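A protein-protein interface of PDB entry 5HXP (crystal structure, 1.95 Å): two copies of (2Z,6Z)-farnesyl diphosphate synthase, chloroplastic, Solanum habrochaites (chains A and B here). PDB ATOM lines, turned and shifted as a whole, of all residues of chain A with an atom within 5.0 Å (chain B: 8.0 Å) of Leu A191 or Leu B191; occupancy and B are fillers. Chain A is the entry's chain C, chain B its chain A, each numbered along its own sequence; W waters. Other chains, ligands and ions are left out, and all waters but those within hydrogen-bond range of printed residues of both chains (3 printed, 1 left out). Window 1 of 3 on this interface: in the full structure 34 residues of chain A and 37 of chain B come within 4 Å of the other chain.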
ATOM      1  N   GLY A 133       4.458 -24.420 -16.768  1.00  0.00           N
ATOM      2  CA  GLY A 133       5.598 -24.407 -15.844  1.00  0.00           C
ATOM      3  C   GLY A 133       6.746 -23.514 -16.287  1.00  0.00           C
ATOM      4  O   GLY A 133       7.333 -22.788 -15.476  1.00  0.00           O
ATOM      5  N   TYR A 134       7.088 -23.552 -17.572  1.00  0.00           N
ATOM      6  CA  TYR A 134       8.110 -22.627 -18.075  1.00  0.00           C
ATOM      7  C   TYR A 134       7.720 -21.193 -17.831  1.00  0.00           C
ATOM      8  O   TYR A 134       8.527 -20.390 -17.330  1.00  0.00           O
ATOM      9  CB  TYR A 134       8.325 -22.776 -19.587  1.00  0.00           C
ATOM     10  CG  TYR A 134       8.732 -24.127 -20.071  1.00  0.00           C
ATOM     11  CD1 TYR A 134       9.722 -24.892 -19.429  1.00  0.00           C
ATOM     12  CD2 TYR A 134       8.167 -24.626 -21.239  1.00  0.00           C
ATOM     13  CE1 TYR A 134      10.102 -26.138 -19.950  1.00  0.00           C
ATOM     14  CE2 TYR A 134       8.520 -25.859 -21.735  1.00  0.00           C
ATOM     15  CZ  TYR A 134       9.474 -26.606 -21.117  1.00  0.00           C
ATOM     16  OH  TYR A 134       9.759 -27.819 -21.732  1.00  0.00           O
ATOM     17  N   ILE A 137       8.049 -20.190 -14.026  1.00  0.00           N
ATOM     18  CA  ILE A 137       9.449 -20.030 -13.652  1.00  0.00           C
ATOM     19  C   ILE A 137      10.041 -18.764 -14.302  1.00  0.00           C
ATOM     20  O   ILE A 137      10.757 -18.010 -13.665  1.00  0.00           O
ATOM     21  CB  ILE A 137      10.247 -21.309 -14.012  1.00  0.00           C
ATOM     22  CG1 ILE A 137       9.846 -22.450 -13.059  1.00  0.00           C
ATOM     23  CG2 ILE A 137      11.737 -21.057 -13.954  1.00  0.00           C
ATOM     24  CD1 ILE A 137      10.179 -23.847 -13.538  1.00  0.00           C
ATOM     25  N   VAL A 186       3.584 -34.824 -17.500  1.00  0.00           N
ATOM     26  CA  VAL A 186       3.043 -33.648 -16.805  1.00  0.00           C
ATOM     27  C   VAL A 186       2.728 -32.484 -17.777  1.00  0.00           C
ATOM     28  O   VAL A 186       2.089 -31.514 -17.395  1.00  0.00           O
ATOM     29  CB  VAL A 186       3.952 -33.156 -15.622  1.00  0.00           C
ATOM     30  CG1 VAL A 186       4.021 -34.184 -14.503  1.00  0.00           C
ATOM     31  CG2 VAL A 186       5.347 -32.801 -16.079  1.00  0.00           C
ATOM     32  N   ASN A 188       4.035 -29.748 -19.058  1.00  0.00           N
ATOM     33  CA  ASN A 188       4.322 -28.356 -18.734  1.00  0.00           C
ATOM     34  C   ASN A 188       3.289 -27.760 -17.772  1.00  0.00           C
ATOM     35  O   ASN A 188       2.972 -26.604 -17.854  1.00  0.00           O
ATOM     36  CB  ASN A 188       4.457 -27.511 -20.017  1.00  0.00           C
ATOM     37  CG  ASN A 188       5.068 -26.139 -19.781  1.00  0.00           C
ATOM     38  OD1 ASN A 188       5.832 -25.914 -18.826  1.00  0.00           O
ATOM     39  ND2 ASN A 188       4.742 -25.200 -20.671  1.00  0.00           N
ATOM     40  N   PHE A 189       2.850 -28.546 -16.799  1.00  0.00           N
ATOM     41  CA  PHE A 189       1.985 -28.068 -15.728  1.00  0.00           C
ATOM     42  C   PHE A 189       2.909 -27.495 -14.616  1.00  0.00           C
ATOM     43  O   PHE A 189       3.873 -26.812 -14.930  1.00  0.00           O
ATOM     44  CB  PHE A 189       1.075 -29.229 -15.294  1.00  0.00           C
ATOM     45  CG  PHE A 189      -0.091 -28.857 -14.395  1.00  0.00           C
ATOM     46  CD1 PHE A 189      -0.675 -27.593 -14.389  1.00  0.00           C
ATOM     47  CD2 PHE A 189      -0.627 -29.822 -13.563  1.00  0.00           C
ATOM     48  CE1 PHE A 189      -1.748 -27.325 -13.557  1.00  0.00           C
ATOM     49  CE2 PHE A 189      -1.679 -29.548 -12.722  1.00  0.00           C
ATOM     50  CZ  PHE A 189      -2.248 -28.299 -12.720  1.00  0.00           C
ATOM     51  N   LEU A 190       2.656 -27.792 -13.346  1.00  0.00           N
ATOM     52  CA  LEU A 190       3.343 -27.132 -12.229  1.00  0.00           C
ATOM     53  C   LEU A 190       4.729 -27.728 -11.917  1.00  0.00           C
ATOM     54  O   LEU A 190       4.931 -28.294 -10.821  1.00  0.00           O
ATOM     55  CB  LEU A 190       2.484 -27.231 -10.972  1.00  0.00           C
ATOM     56  CG  LEU A 190       0.991 -26.929 -11.088  1.00  0.00           C
ATOM     57  CD1 LEU A 190       0.277 -27.410  -9.831  1.00  0.00           C
ATOM     58  CD2 LEU A 190       0.762 -25.452 -11.344  1.00  0.00           C
ATOM     59  N   LEU A 191       5.677 -27.539 -12.830  1.00  0.00           N
ATOM     60  CA  LEU A 191       6.973 -28.254 -12.798  1.00  0.00           C
ATOM     61  C   LEU A 191       7.744 -28.121 -11.478  1.00  0.00           C
ATOM     62  O   LEU A 191       8.112 -29.121 -10.886  1.00  0.00           O
ATOM     63  CB  LEU A 191       7.869 -27.790 -13.932  1.00  0.00           C
ATOM     64  CG  LEU A 191       7.250 -27.924 -15.314  1.00  0.00           C
ATOM     65  CD1 LEU A 191       8.158 -27.242 -16.311  1.00  0.00           C
ATOM     66  CD2 LEU A 191       6.983 -29.388 -15.645  1.00  0.00           C
ATOM     67  N   TRP A 192       8.000 -26.900 -11.030  1.00  0.00           N
ATOM     68  CA  TRP A 192       8.691 -26.689  -9.748  1.00  0.00           C
ATOM     69  C   TRP A 192       7.916 -27.311  -8.619  1.00  0.00           C
ATOM     70  O   TRP A 192       8.488 -27.978  -7.745  1.00  0.00           O
ATOM     71  CB  TRP A 192       8.865 -25.194  -9.468  1.00  0.00           C
ATOM     72  CG  TRP A 192       9.398 -24.784  -8.105  1.00  0.00           C
ATOM     73  CD1 TRP A 192       8.687 -24.709  -6.914  1.00  0.00           C
ATOM     74  CD2 TRP A 192      10.708 -24.304  -7.810  1.00  0.00           C
ATOM     75  NE1 TRP A 192       9.478 -24.218  -5.927  1.00  0.00           N
ATOM     76  CE2 TRP A 192      10.730 -23.976  -6.429  1.00  0.00           C
ATOM     77  CE3 TRP A 192      11.881 -24.156  -8.562  1.00  0.00           C
ATOM     78  CZ2 TRP A 192      11.872 -23.478  -5.803  1.00  0.00           C
ATOM     79  CZ3 TRP A 192      13.000 -23.665  -7.955  1.00  0.00           C
ATOM     80  CH2 TRP A 192      13.002 -23.331  -6.580  1.00  0.00           C
ATOM     81  N   GLN A 193       6.607 -27.094  -8.655  1.00  0.00           N
ATOM     82  CA  GLN A 193       5.719 -27.413  -7.549  1.00  0.00           C
ATOM     83  C   GLN A 193       5.475 -28.926  -7.446  1.00  0.00           C
ATOM     84  O   GLN A 193       5.061 -29.434  -6.403  1.00  0.00           O
ATOM     85  CB  GLN A 193       4.391 -26.638  -7.683  1.00  0.00           C
ATOM     86  CG  GLN A 193       4.512 -25.105  -7.657  1.00  0.00           C
ATOM     87  CD  GLN A 193       4.804 -24.463  -9.023  1.00  0.00           C
ATOM     88  OE1 GLN A 193       5.165 -25.133  -9.985  1.00  0.00           O
ATOM     89  NE2 GLN A 193       4.634 -23.161  -9.098  1.00  0.00           N
ATOM     90  N   LEU A 194       5.774 -29.656  -8.514  1.00  0.00           N
ATOM     91  CA  LEU A 194       5.551 -31.080  -8.531  1.00  0.00           C
ATOM     92  C   LEU A 194       6.759 -31.884  -8.115  1.00  0.00           C
ATOM     93  O   LEU A 194       6.693 -33.096  -8.218  1.00  0.00           O
ATOM     94  CB  LEU A 194       5.070 -31.541  -9.919  1.00  0.00           C
ATOM     95  CG  LEU A 194       3.651 -31.103 -10.271  1.00  0.00           C
ATOM     96  CD1 LEU A 194       3.394 -31.322 -11.762  1.00  0.00           C
ATOM     97  CD2 LEU A 194       2.639 -31.856  -9.431  1.00  0.00           C
ATOM     98  N   ALA A 195       7.811 -31.236  -7.592  1.00  0.00           N
ATOM     99  CA  ALA A 195       9.087 -31.911  -7.279  1.00  0.00           C
ATOM    100  C   ALA A 195       8.982 -33.168  -6.408  1.00  0.00           C
ATOM    101  O   ALA A 195       9.742 -34.101  -6.622  1.00  0.00           O
ATOM    102  CB  ALA A 195      10.069 -30.919  -6.646  1.00  0.00           C
ATOM    103  N   TYR B 131      22.494 -33.399  -6.807  1.00  0.00           N
ATOM    104  CA  TYR B 131      21.759 -32.581  -7.724  1.00  0.00           C
ATOM    105  C   TYR B 131      20.322 -32.463  -7.238  1.00  0.00           C
ATOM    106  O   TYR B 131      19.769 -33.400  -6.648  1.00  0.00           O
ATOM    107  CB  TYR B 131      21.805 -33.204  -9.137  1.00  0.00           C
ATOM    108  CG  TYR B 131      20.960 -32.460 -10.129  1.00  0.00           C
ATOM    109  CD1 TYR B 131      21.469 -31.387 -10.840  1.00  0.00           C
ATOM    110  CD2 TYR B 131      19.628 -32.818 -10.330  1.00  0.00           C
ATOM    111  CE1 TYR B 131      20.678 -30.692 -11.751  1.00  0.00           C
ATOM    112  CE2 TYR B 131      18.835 -32.135 -11.230  1.00  0.00           C
ATOM    113  CZ  TYR B 131      19.355 -31.079 -11.926  1.00  0.00           C
ATOM    114  OH  TYR B 131      18.538 -30.411 -12.801  1.00  0.00           O
ATOM    115  N   GLY B 132      19.721 -31.316  -7.526  1.00  0.00           N
ATOM    116  CA  GLY B 132      18.279 -31.129  -7.390  1.00  0.00           C
ATOM    117  C   GLY B 132      17.752 -30.165  -8.430  1.00  0.00           C
ATOM    118  O   GLY B 132      18.407 -29.168  -8.750  1.00  0.00           O
ATOM    119  N   GLY B 133      16.565 -30.448  -8.968  1.00  0.00           N
ATOM    120  CA  GLY B 133      15.907 -29.524  -9.871  1.00  0.00           C
ATOM    121  C   GLY B 133      15.824 -28.106  -9.335  1.00  0.00           C
ATOM    122  O   GLY B 133      16.084 -27.160 -10.069  1.00  0.00           O
ATOM    123  N   TYR B 134      15.480 -27.951  -8.051  1.00  0.00           N
ATOM    124  CA  TYR B 134      15.365 -26.616  -7.473  1.00  0.00           C
ATOM    125  C   TYR B 134      16.684 -25.880  -7.595  1.00  0.00           C
ATOM    126  O   TYR B 134      16.739 -24.712  -7.940  1.00  0.00           O
ATOM    127  CB  TYR B 134      15.065 -26.661  -5.993  1.00  0.00           C
ATOM    128  CG  TYR B 134      13.780 -27.287  -5.550  1.00  0.00           C
ATOM    129  CD1 TYR B 134      12.560 -27.077  -6.214  1.00  0.00           C
ATOM    130  CD2 TYR B 134      13.772 -28.020  -4.386  1.00  0.00           C
ATOM    131  CE1 TYR B 134      11.376 -27.644  -5.728  1.00  0.00           C
ATOM    132  CE2 TYR B 134      12.615 -28.568  -3.884  1.00  0.00           C
ATOM    133  CZ  TYR B 134      11.437 -28.392  -4.532  1.00  0.00           C
ATOM    134  OH  TYR B 134      10.355 -28.993  -3.930  1.00  0.00           O
ATOM    135  N   TYR B 135      17.750 -26.596  -7.309  1.00  0.00           N
ATOM    136  CA  TYR B 135      19.063 -25.999  -7.264  1.00  0.00           C
ATOM    137  C   TYR B 135      19.568 -25.656  -8.680  1.00  0.00           C
ATOM    138  O   TYR B 135      20.197 -24.632  -8.866  1.00  0.00           O
ATOM    139  CB  TYR B 135      19.947 -26.894  -6.385  1.00  0.00           C
ATOM    140  CG  TYR B 135      19.193 -27.070  -5.054  1.00  0.00           C
ATOM    141  CD1 TYR B 135      18.489 -28.249  -4.763  1.00  0.00           C
ATOM    142  CD2 TYR B 135      19.041 -25.995  -4.185  1.00  0.00           C
ATOM    143  CE1 TYR B 135      17.759 -28.363  -3.588  1.00  0.00           C
ATOM    144  CE2 TYR B 135      18.311 -26.103  -3.012  1.00  0.00           C
ATOM    145  CZ  TYR B 135      17.678 -27.283  -2.713  1.00  0.00           C
ATOM    146  OH  TYR B 135      16.940 -27.388  -1.543  1.00  0.00           O
ATOM    147  N   ASP B 136      19.210 -26.466  -9.676  1.00  0.00           N
ATOM    148  CA  ASP B 136      19.542 -26.165 -11.079  1.00  0.00           C
ATOM    149  C   ASP B 136      18.860 -24.873 -11.534  1.00  0.00           C
ATOM    150  O   ASP B 136      19.517 -23.963 -12.078  1.00  0.00           O
ATOM    151  CB  ASP B 136      19.154 -27.368 -11.963  1.00  0.00           C
ATOM    152  CG  ASP B 136      19.789 -27.333 -13.340  1.00  0.00           C
ATOM    153  OD1 ASP B 136      20.594 -26.413 -13.636  1.00  0.00           O
ATOM    154  OD2 ASP B 136      19.471 -28.253 -14.136  1.00  0.00           O
ATOM    155  N   ILE B 137      17.553 -24.775 -11.279  1.00  0.00           N
ATOM    156  CA  ILE B 137      16.768 -23.571 -11.563  1.00  0.00           C
ATOM    157  C   ILE B 137      17.313 -22.356 -10.799  1.00  0.00           C
ATOM    158  O   ILE B 137      17.464 -21.263 -11.379  1.00  0.00           O
ATOM    159  CB  ILE B 137      15.274 -23.799 -11.269  1.00  0.00           C
ATOM    160  CG1 ILE B 137      14.681 -24.726 -12.353  1.00  0.00           C
ATOM    161  CG2 ILE B 137      14.492 -22.501 -11.185  1.00  0.00           C
ATOM    162  CD1 ILE B 137      13.446 -25.474 -11.911  1.00  0.00           C
ATOM    163  N   LEU B 167      20.815 -23.685 -17.594  1.00  0.00           N
ATOM    164  CA  LEU B 167      20.614 -24.880 -16.753  1.00  0.00           C
ATOM    165  C   LEU B 167      21.767 -25.858 -16.962  1.00  0.00           C
ATOM    166  O   LEU B 167      22.433 -25.809 -17.996  1.00  0.00           O
ATOM    167  CB  LEU B 167      19.267 -25.537 -17.074  1.00  0.00           C
ATOM    168  CG  LEU B 167      18.046 -24.768 -16.560  1.00  0.00           C
ATOM    169  CD1 LEU B 167      16.792 -25.156 -17.322  1.00  0.00           C
ATOM    170  CD2 LEU B 167      17.848 -25.005 -15.076  1.00  0.00           C
ATOM    171  N   SER B 169      21.586 -29.355 -16.890  1.00  0.00           N
ATOM    172  CA  SER B 169      21.131 -30.388 -17.833  1.00  0.00           C
ATOM    173  C   SER B 169      20.546 -29.708 -19.076  1.00  0.00           C
ATOM    174  O   SER B 169      19.511 -29.036 -19.002  1.00  0.00           O
ATOM    175  CB  SER B 169      20.103 -31.329 -17.204  1.00  0.00           C
ATOM    176  OG  SER B 169      19.570 -32.223 -18.176  1.00  0.00           O
ATOM    177  N   ASN B 173      16.187 -32.437 -24.215  1.00  0.00           N
ATOM    178  CA  ASN B 173      15.670 -32.977 -22.966  1.00  0.00           C
ATOM    179  C   ASN B 173      15.309 -34.455 -23.069  1.00  0.00           C
ATOM    180  O   ASN B 173      15.193 -34.995 -24.173  1.00  0.00           O
ATOM    181  CB  ASN B 173      14.460 -32.169 -22.540  1.00  0.00           C
ATOM    182  CG  ASN B 173      14.811 -30.732 -22.202  1.00  0.00           C
ATOM    183  OD1 ASN B 173      15.901 -30.417 -21.700  1.00  0.00           O
ATOM    184  ND2 ASN B 173      13.889 -29.860 -22.475  1.00  0.00           N
ATOM    185  N   VAL B 186       9.069 -37.645  -9.160  1.00  0.00           N
ATOM    186  CA  VAL B 186      10.359 -37.242  -9.748  1.00  0.00           C
ATOM    187  C   VAL B 186      11.417 -36.903  -8.690  1.00  0.00           C
ATOM    188  O   VAL B 186      12.607 -36.836  -9.009  1.00  0.00           O
ATOM    189  CB  VAL B 186      10.215 -36.094 -10.779  1.00  0.00           C
ATOM    190  CG1 VAL B 186       9.372 -36.564 -11.959  1.00  0.00           C
ATOM    191  CG2 VAL B 186       9.599 -34.834 -10.176  1.00  0.00           C
ATOM    192  N   SER B 187      10.985 -36.693  -7.447  1.00  0.00           N
ATOM    193  CA  SER B 187      11.896 -36.468  -6.321  1.00  0.00           C
ATOM    194  C   SER B 187      12.955 -35.396  -6.596  1.00  0.00           C
ATOM    195  O   SER B 187      14.115 -35.599  -6.313  1.00  0.00           O
ATOM    196  CB  SER B 187      12.566 -37.793  -5.920  1.00  0.00           C
ATOM    197  OG  SER B 187      11.595 -38.697  -5.438  1.00  0.00           O
ATOM    198  N   ASN B 188      12.550 -34.253  -7.127  1.00  0.00           N
ATOM    199  CA  ASN B 188      13.463 -33.124  -7.343  1.00  0.00           C
ATOM    200  C   ASN B 188      14.635 -33.439  -8.279  1.00  0.00           C
ATOM    201  O   ASN B 188      15.754 -32.963  -8.062  1.00  0.00           O
ATOM    202  CB  ASN B 188      13.994 -32.592  -5.998  1.00  0.00           C
ATOM    203  CG  ASN B 188      14.604 -31.201  -6.107  1.00  0.00           C
ATOM    204  OD1 ASN B 188      14.295 -30.434  -7.022  1.00  0.00           O
ATOM    205  ND2 ASN B 188      15.502 -30.873  -5.162  1.00  0.00           N
ATOM    206  N   PHE B 189      14.359 -34.225  -9.330  1.00  0.00           N
ATOM    207  CA  PHE B 189      15.325 -34.498 -10.396  1.00  0.00           C
ATOM    208  C   PHE B 189      15.201 -33.337 -11.390  1.00  0.00           C
ATOM    209  O   PHE B 189      15.025 -32.205 -10.978  1.00  0.00           O
ATOM    210  CB  PHE B 189      14.991 -35.874 -10.985  1.00  0.00           C
ATOM    211  CG  PHE B 189      16.024 -36.463 -11.927  1.00  0.00           C
ATOM    212  CD1 PHE B 189      17.378 -36.131 -11.882  1.00  0.00           C
ATOM    213  CD2 PHE B 189      15.606 -37.419 -12.857  1.00  0.00           C
ATOM    214  CE1 PHE B 189      18.285 -36.729 -12.761  1.00  0.00           C
ATOM    215  CE2 PHE B 189      16.505 -38.032 -13.700  1.00  0.00           C
ATOM    216  CZ  PHE B 189      17.847 -37.683 -13.660  1.00  0.00           C
ATOM    217  N   LEU B 190      15.194 -33.610 -12.684  1.00  0.00           N
ATOM    218  CA  LEU B 190      15.207 -32.592 -13.741  1.00  0.00           C
ATOM    219  C   LEU B 190      13.871 -31.889 -14.043  1.00  0.00           C
ATOM    220  O   LEU B 190      13.271 -32.092 -15.127  1.00  0.00           O
ATOM    221  CB  LEU B 190      15.632 -33.273 -15.015  1.00  0.00           C
ATOM    222  CG  LEU B 190      16.884 -34.114 -14.993  1.00  0.00           C
ATOM    223  CD1 LEU B 190      16.943 -34.856 -16.315  1.00  0.00           C
ATOM    224  CD2 LEU B 190      18.098 -33.236 -14.775  1.00  0.00           C
ATOM    225  N   LEU B 191      13.458 -30.998 -13.163  1.00  0.00           N
ATOM    226  CA  LEU B 191      12.095 -30.433 -13.187  1.00  0.00           C
ATOM    227  C   LEU B 191      11.741 -29.697 -14.498  1.00  0.00           C
ATOM    228  O   LEU B 191      10.769 -30.014 -15.163  1.00  0.00           O
ATOM    229  CB  LEU B 191      11.933 -29.499 -11.990  1.00  0.00           C
ATOM    230  CG  LEU B 191      12.114 -30.211 -10.634  1.00  0.00           C
ATOM    231  CD1 LEU B 191      12.060 -29.201  -9.502  1.00  0.00           C
ATOM    232  CD2 LEU B 191      11.082 -31.319 -10.432  1.00  0.00           C
ATOM    233  N   TRP B 192      12.541 -28.712 -14.843  1.00  0.00           N
ATOM    234  CA  TRP B 192      12.326 -27.933 -16.065  1.00  0.00           C
ATOM    235  C   TRP B 192      12.464 -28.849 -17.278  1.00  0.00           C
ATOM    236  O   TRP B 192      11.638 -28.817 -18.183  1.00  0.00           O
ATOM    237  CB  TRP B 192      13.343 -26.805 -16.110  1.00  0.00           C
ATOM    238  CG  TRP B 192      13.399 -26.034 -17.400  1.00  0.00           C
ATOM    239  CD1 TRP B 192      13.977 -26.439 -18.577  1.00  0.00           C
ATOM    240  CD2 TRP B 192      12.934 -24.716 -17.610  1.00  0.00           C
ATOM    241  NE1 TRP B 192      13.874 -25.451 -19.512  1.00  0.00           N
ATOM    242  CE2 TRP B 192      13.234 -24.378 -18.953  1.00  0.00           C
ATOM    243  CE3 TRP B 192      12.271 -23.785 -16.813  1.00  0.00           C
ATOM    244  CZ2 TRP B 192      12.888 -23.152 -19.502  1.00  0.00           C
ATOM    245  CZ3 TRP B 192      11.918 -22.558 -17.373  1.00  0.00           C
ATOM    246  CH2 TRP B 192      12.244 -22.243 -18.682  1.00  0.00           C
ATOM    247  N   GLN B 193      13.464 -29.724 -17.246  1.00  0.00           N
ATOM    248  CA  GLN B 193      13.777 -30.582 -18.386  1.00  0.00           C
ATOM    249  C   GLN B 193      12.784 -31.707 -18.646  1.00  0.00           C
ATOM    250  O   GLN B 193      12.822 -32.323 -19.710  1.00  0.00           O
ATOM    251  CB  GLN B 193      15.176 -31.187 -18.217  1.00  0.00           C
ATOM    252  CG  GLN B 193      16.280 -30.166 -18.142  1.00  0.00           C
ATOM    253  CD  GLN B 193      16.583 -29.614 -16.749  1.00  0.00           C
ATOM    254  OE1 GLN B 193      15.794 -29.713 -15.812  1.00  0.00           O
ATOM    255  NE2 GLN B 193      17.742 -28.989 -16.629  1.00  0.00           N
ATOM    256  N   LEU B 194      11.890 -31.974 -17.699  1.00  0.00           N
ATOM    257  CA  LEU B 194      10.956 -33.072 -17.810  1.00  0.00           C
ATOM    258  C   LEU B 194       9.562 -32.636 -18.279  1.00  0.00           C
ATOM    259  O   LEU B 194       8.619 -33.443 -18.269  1.00  0.00           O
ATOM    260  CB  LEU B 194      10.866 -33.789 -16.459  1.00  0.00           C
ATOM    261  CG  LEU B 194      12.109 -34.620 -16.101  1.00  0.00           C
ATOM    262  CD1 LEU B 194      11.973 -35.183 -14.683  1.00  0.00           C
ATOM    263  CD2 LEU B 194      12.370 -35.744 -17.101  1.00  0.00           C
ATOM    264  N   ALA B 195       9.430 -31.397 -18.740  1.00  0.00           N
ATOM    265  CA  ALA B 195       8.106 -30.806 -19.008  1.00  0.00           C
ATOM    266  C   ALA B 195       7.208 -31.664 -19.919  1.00  0.00           C
ATOM    267  O   ALA B 195       5.998 -31.736 -19.700  1.00  0.00           O
ATOM    268  CB  ALA B 195       8.259 -29.402 -19.588  1.00  0.00           C
ATOM    269  N   TYR B 196       7.811 -32.333 -20.905  1.00  0.00           N
ATOM    270  CA  TYR B 196       7.055 -33.162 -21.858  1.00  0.00           C
ATOM    271  C   TYR B 196       7.602 -34.578 -22.008  1.00  0.00           C
ATOM    272  O   TYR B 196       7.219 -35.327 -22.930  1.00  0.00           O
ATOM    273  CB  TYR B 196       6.932 -32.448 -23.217  1.00  0.00           C
ATOM    274  CG  TYR B 196       5.797 -31.447 -23.253  1.00  0.00           C
ATOM    275  CD1 TYR B 196       4.477 -31.873 -23.308  1.00  0.00           C
ATOM    276  CD2 TYR B 196       6.037 -30.082 -23.245  1.00  0.00           C
ATOM    277  CE1 TYR B 196       3.430 -30.973 -23.331  1.00  0.00           C
ATOM    278  CE2 TYR B 196       4.990 -29.175 -23.265  1.00  0.00           C
ATOM    279  CZ  TYR B 196       3.685 -29.629 -23.324  1.00  0.00           C
ATOM    280  OH  TYR B 196       2.612 -28.737 -23.329  1.00  0.00           O
ATOM    281  N   THR B 197       8.464 -34.964 -21.066  1.00  0.00           N
ATOM    282  CA  THR B 197       8.997 -36.313 -20.992  1.00  0.00           C
ATOM    283  C   THR B 197       7.930 -37.364 -20.687  1.00  0.00           C
ATOM    284  O   THR B 197       7.057 -37.143 -19.869  1.00  0.00           O
ATOM    285  CB  THR B 197      10.111 -36.379 -19.924  1.00  0.00           C
ATOM    286  OG1 THR B 197      11.128 -35.424 -20.257  1.00  0.00           O
ATOM    287  CG2 THR B 197      10.719 -37.770 -19.855  1.00  0.00           C
ATOM    288  N   PHE B 199       6.910 -40.694 -18.830  1.00  0.00           N
ATOM    289  CA  PHE B 199       7.312 -41.352 -17.595  1.00  0.00           C
ATOM    290  C   PHE B 199       7.026 -42.844 -17.622  1.00  0.00           C
ATOM    291  O   PHE B 199       5.939 -43.263 -18.028  1.00  0.00           O
ATOM    292  CB  PHE B 199       6.557 -40.785 -16.391  1.00  0.00           C
ATOM    293  CG  PHE B 199       6.762 -39.308 -16.144  1.00  0.00           C
ATOM    294  CD1 PHE B 199       7.815 -38.612 -16.680  1.00  0.00           C
ATOM    295  CD2 PHE B 199       5.885 -38.629 -15.318  1.00  0.00           C
ATOM    296  CE1 PHE B 199       7.985 -37.254 -16.414  1.00  0.00           C
ATOM    297  CE2 PHE B 199       6.043 -37.273 -15.057  1.00  0.00           C
ATOM    298  CZ  PHE B 199       7.108 -36.589 -15.599  1.00  0.00           C
HETATM  299  O   HOH W   1      11.682 -29.306 -20.902  1.00  0.00           O
HETATM  300  O   HOH W   2       7.324 -35.838  -7.877  1.00  0.00           O
HETATM  301  O   HOH W   3       8.042 -28.450  -4.926  1.00  0.00           O
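Among the printed residues, pairs that only touch across the chains: Tyr A134 with Ala B195 (3.1 Å), Ala A195 with Tyr B134 (3.3 Å), Trp A192 with Tyr B134 (3.5 Å), Tyr A134 with Trp B192 (3.6 Å), Ala A195 with Val B186 (3.6 Å), Asn A188 with Tyr B196 (3.7 Å), Leu A191 with Leu B191 (3.7 Å), Val A186 with Phe B199 (3.7 Å), Ile A137 with Trp B192 (3.7 Å), Trp A192 with Ile B137 (3.7 Å), Ala A195 with Leu B191 (3.8 Å), Leu A191 with Ala B195 (3.8 Å), Val A186 with Ala B195 (3.8 Å), Leu A194 with Val B186 (3.9 Å), Val A186 with Leu B194 (3.99 Å) and Ile A137 with Ile B137 (3.996 Å).
O of Ala A195 sits at hydrogen-bond distance from N of Asn B188.
The backbone NH (N) of Ser B187 is in hydrogen-bond range of the backbone carbonyl oxygen (O) of Ala A195 (3.0 Å).
The backbone carbonyl oxygen of Ala B195 lies within hydrogen-bond range of the backbone NH of Asn A188.
Ile B137 touches its own counterpart, Ile A137.
Ile A137 touches Trp B192, and with the chains exchanged Trp A192 touches Ile B137.
Val A186 touches Leu B194, and with the chains exchanged Leu A194 touches Val B186.
Asn A188 touches Ala B195, and with the chains exchanged Ala A195 touches Asn B188.
Water W1 lies within hydrogen-bond range of OH of Tyr A134 (2.6 Å), O of Trp B192 (2.8 Å), ND2 of Asn B173 (2.8 Å) and O of Gln B193 (3.4 Å).
Water W3 lies within hydrogen-bond range of OH of Tyr B134 (2.6 Å), O of Trp A192 (2.9 Å) and O of Gln A193 (3.5 Å).
Water W2 lies within hydrogen-bond range of the backbone NH (N) of Val B186 (2.8 Å), the backbone carbonyl oxygen (O) of Leu A194 (2.8 Å) and the backbone carbonyl oxygen (O) of Ala A195 (3.2 Å).
Printed residues of chain B within 4 Å of Leu A191: Leu B191 and Ala B195.
Leu B191 touches just these residues of chain A: Leu A191 and Ala A195.
Of the printed residues of chain A, Ser B187 touches Ala A195 (3.0 Å).
Printed residues of chain A within 4 Å of Ala B195: Tyr A134, Val A186, Asn A188 and Leu A191.
Of the printed residues of chain B, Val A186 touches Leu B194, Ala B195 and Phe B199.
Printed residues of chain A within 4 Å of Tyr B134: Trp A192 and Ala A195.
Gln B193 touches none of the printed residues of chain A.
Gly B133 touches none of the printed residues of chain A.
The nearest residue of chain B that does not touch Leu A191 is Trp B192 (4.2 Å).
The nearest printed residue of chain A that does not touch Leu B194 is Leu A191 (4.9 Å).
The backbone NH (N) of Tyr B134 is in hydrogen-bond range of the side-chain amide oxygen (OD1) of Asn B188 (2.9 Å).
The side-chain amide oxygen (OD1) of Asn A188 sits at hydrogen-bond distance from the backbone NH (N) of Tyr A134 (3.0 Å).
N of Gly A133 lies within hydrogen-bond range of O of Asn A188, 2.9 Å away.
The backbone NH (N) of Gly B133 sits at hydrogen-bond distance from the backbone carbonyl oxygen (O) of Asn B188, 2.8 Å away.
Of the 23 printed residues of chain B, 11 touch a printed residue of chain A.
Hydrophobic or aromatic side chains of chain B within 4 Å of the printed part of chain A: Tyr B134, Ile B137, Val B186, Leu B191, Trp B192, Ala B195, Tyr B196 and Phe B199.
Of the 12 printed residues of chain A, 8 touch a printed residue of chain B.
Hydrophobic or aromatic side chains of chain A that line the printed part of chain B: Tyr A134, Ile A137, Val A186, Leu A191, Trp A192 and Ala A195.
Among the printed residues, 19 pairs touch across the chains.
Among the printed residues, no Asp or Glu carboxylate lies within 4 Å of a Lys or Arg side-chain nitrogen of the other chain.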
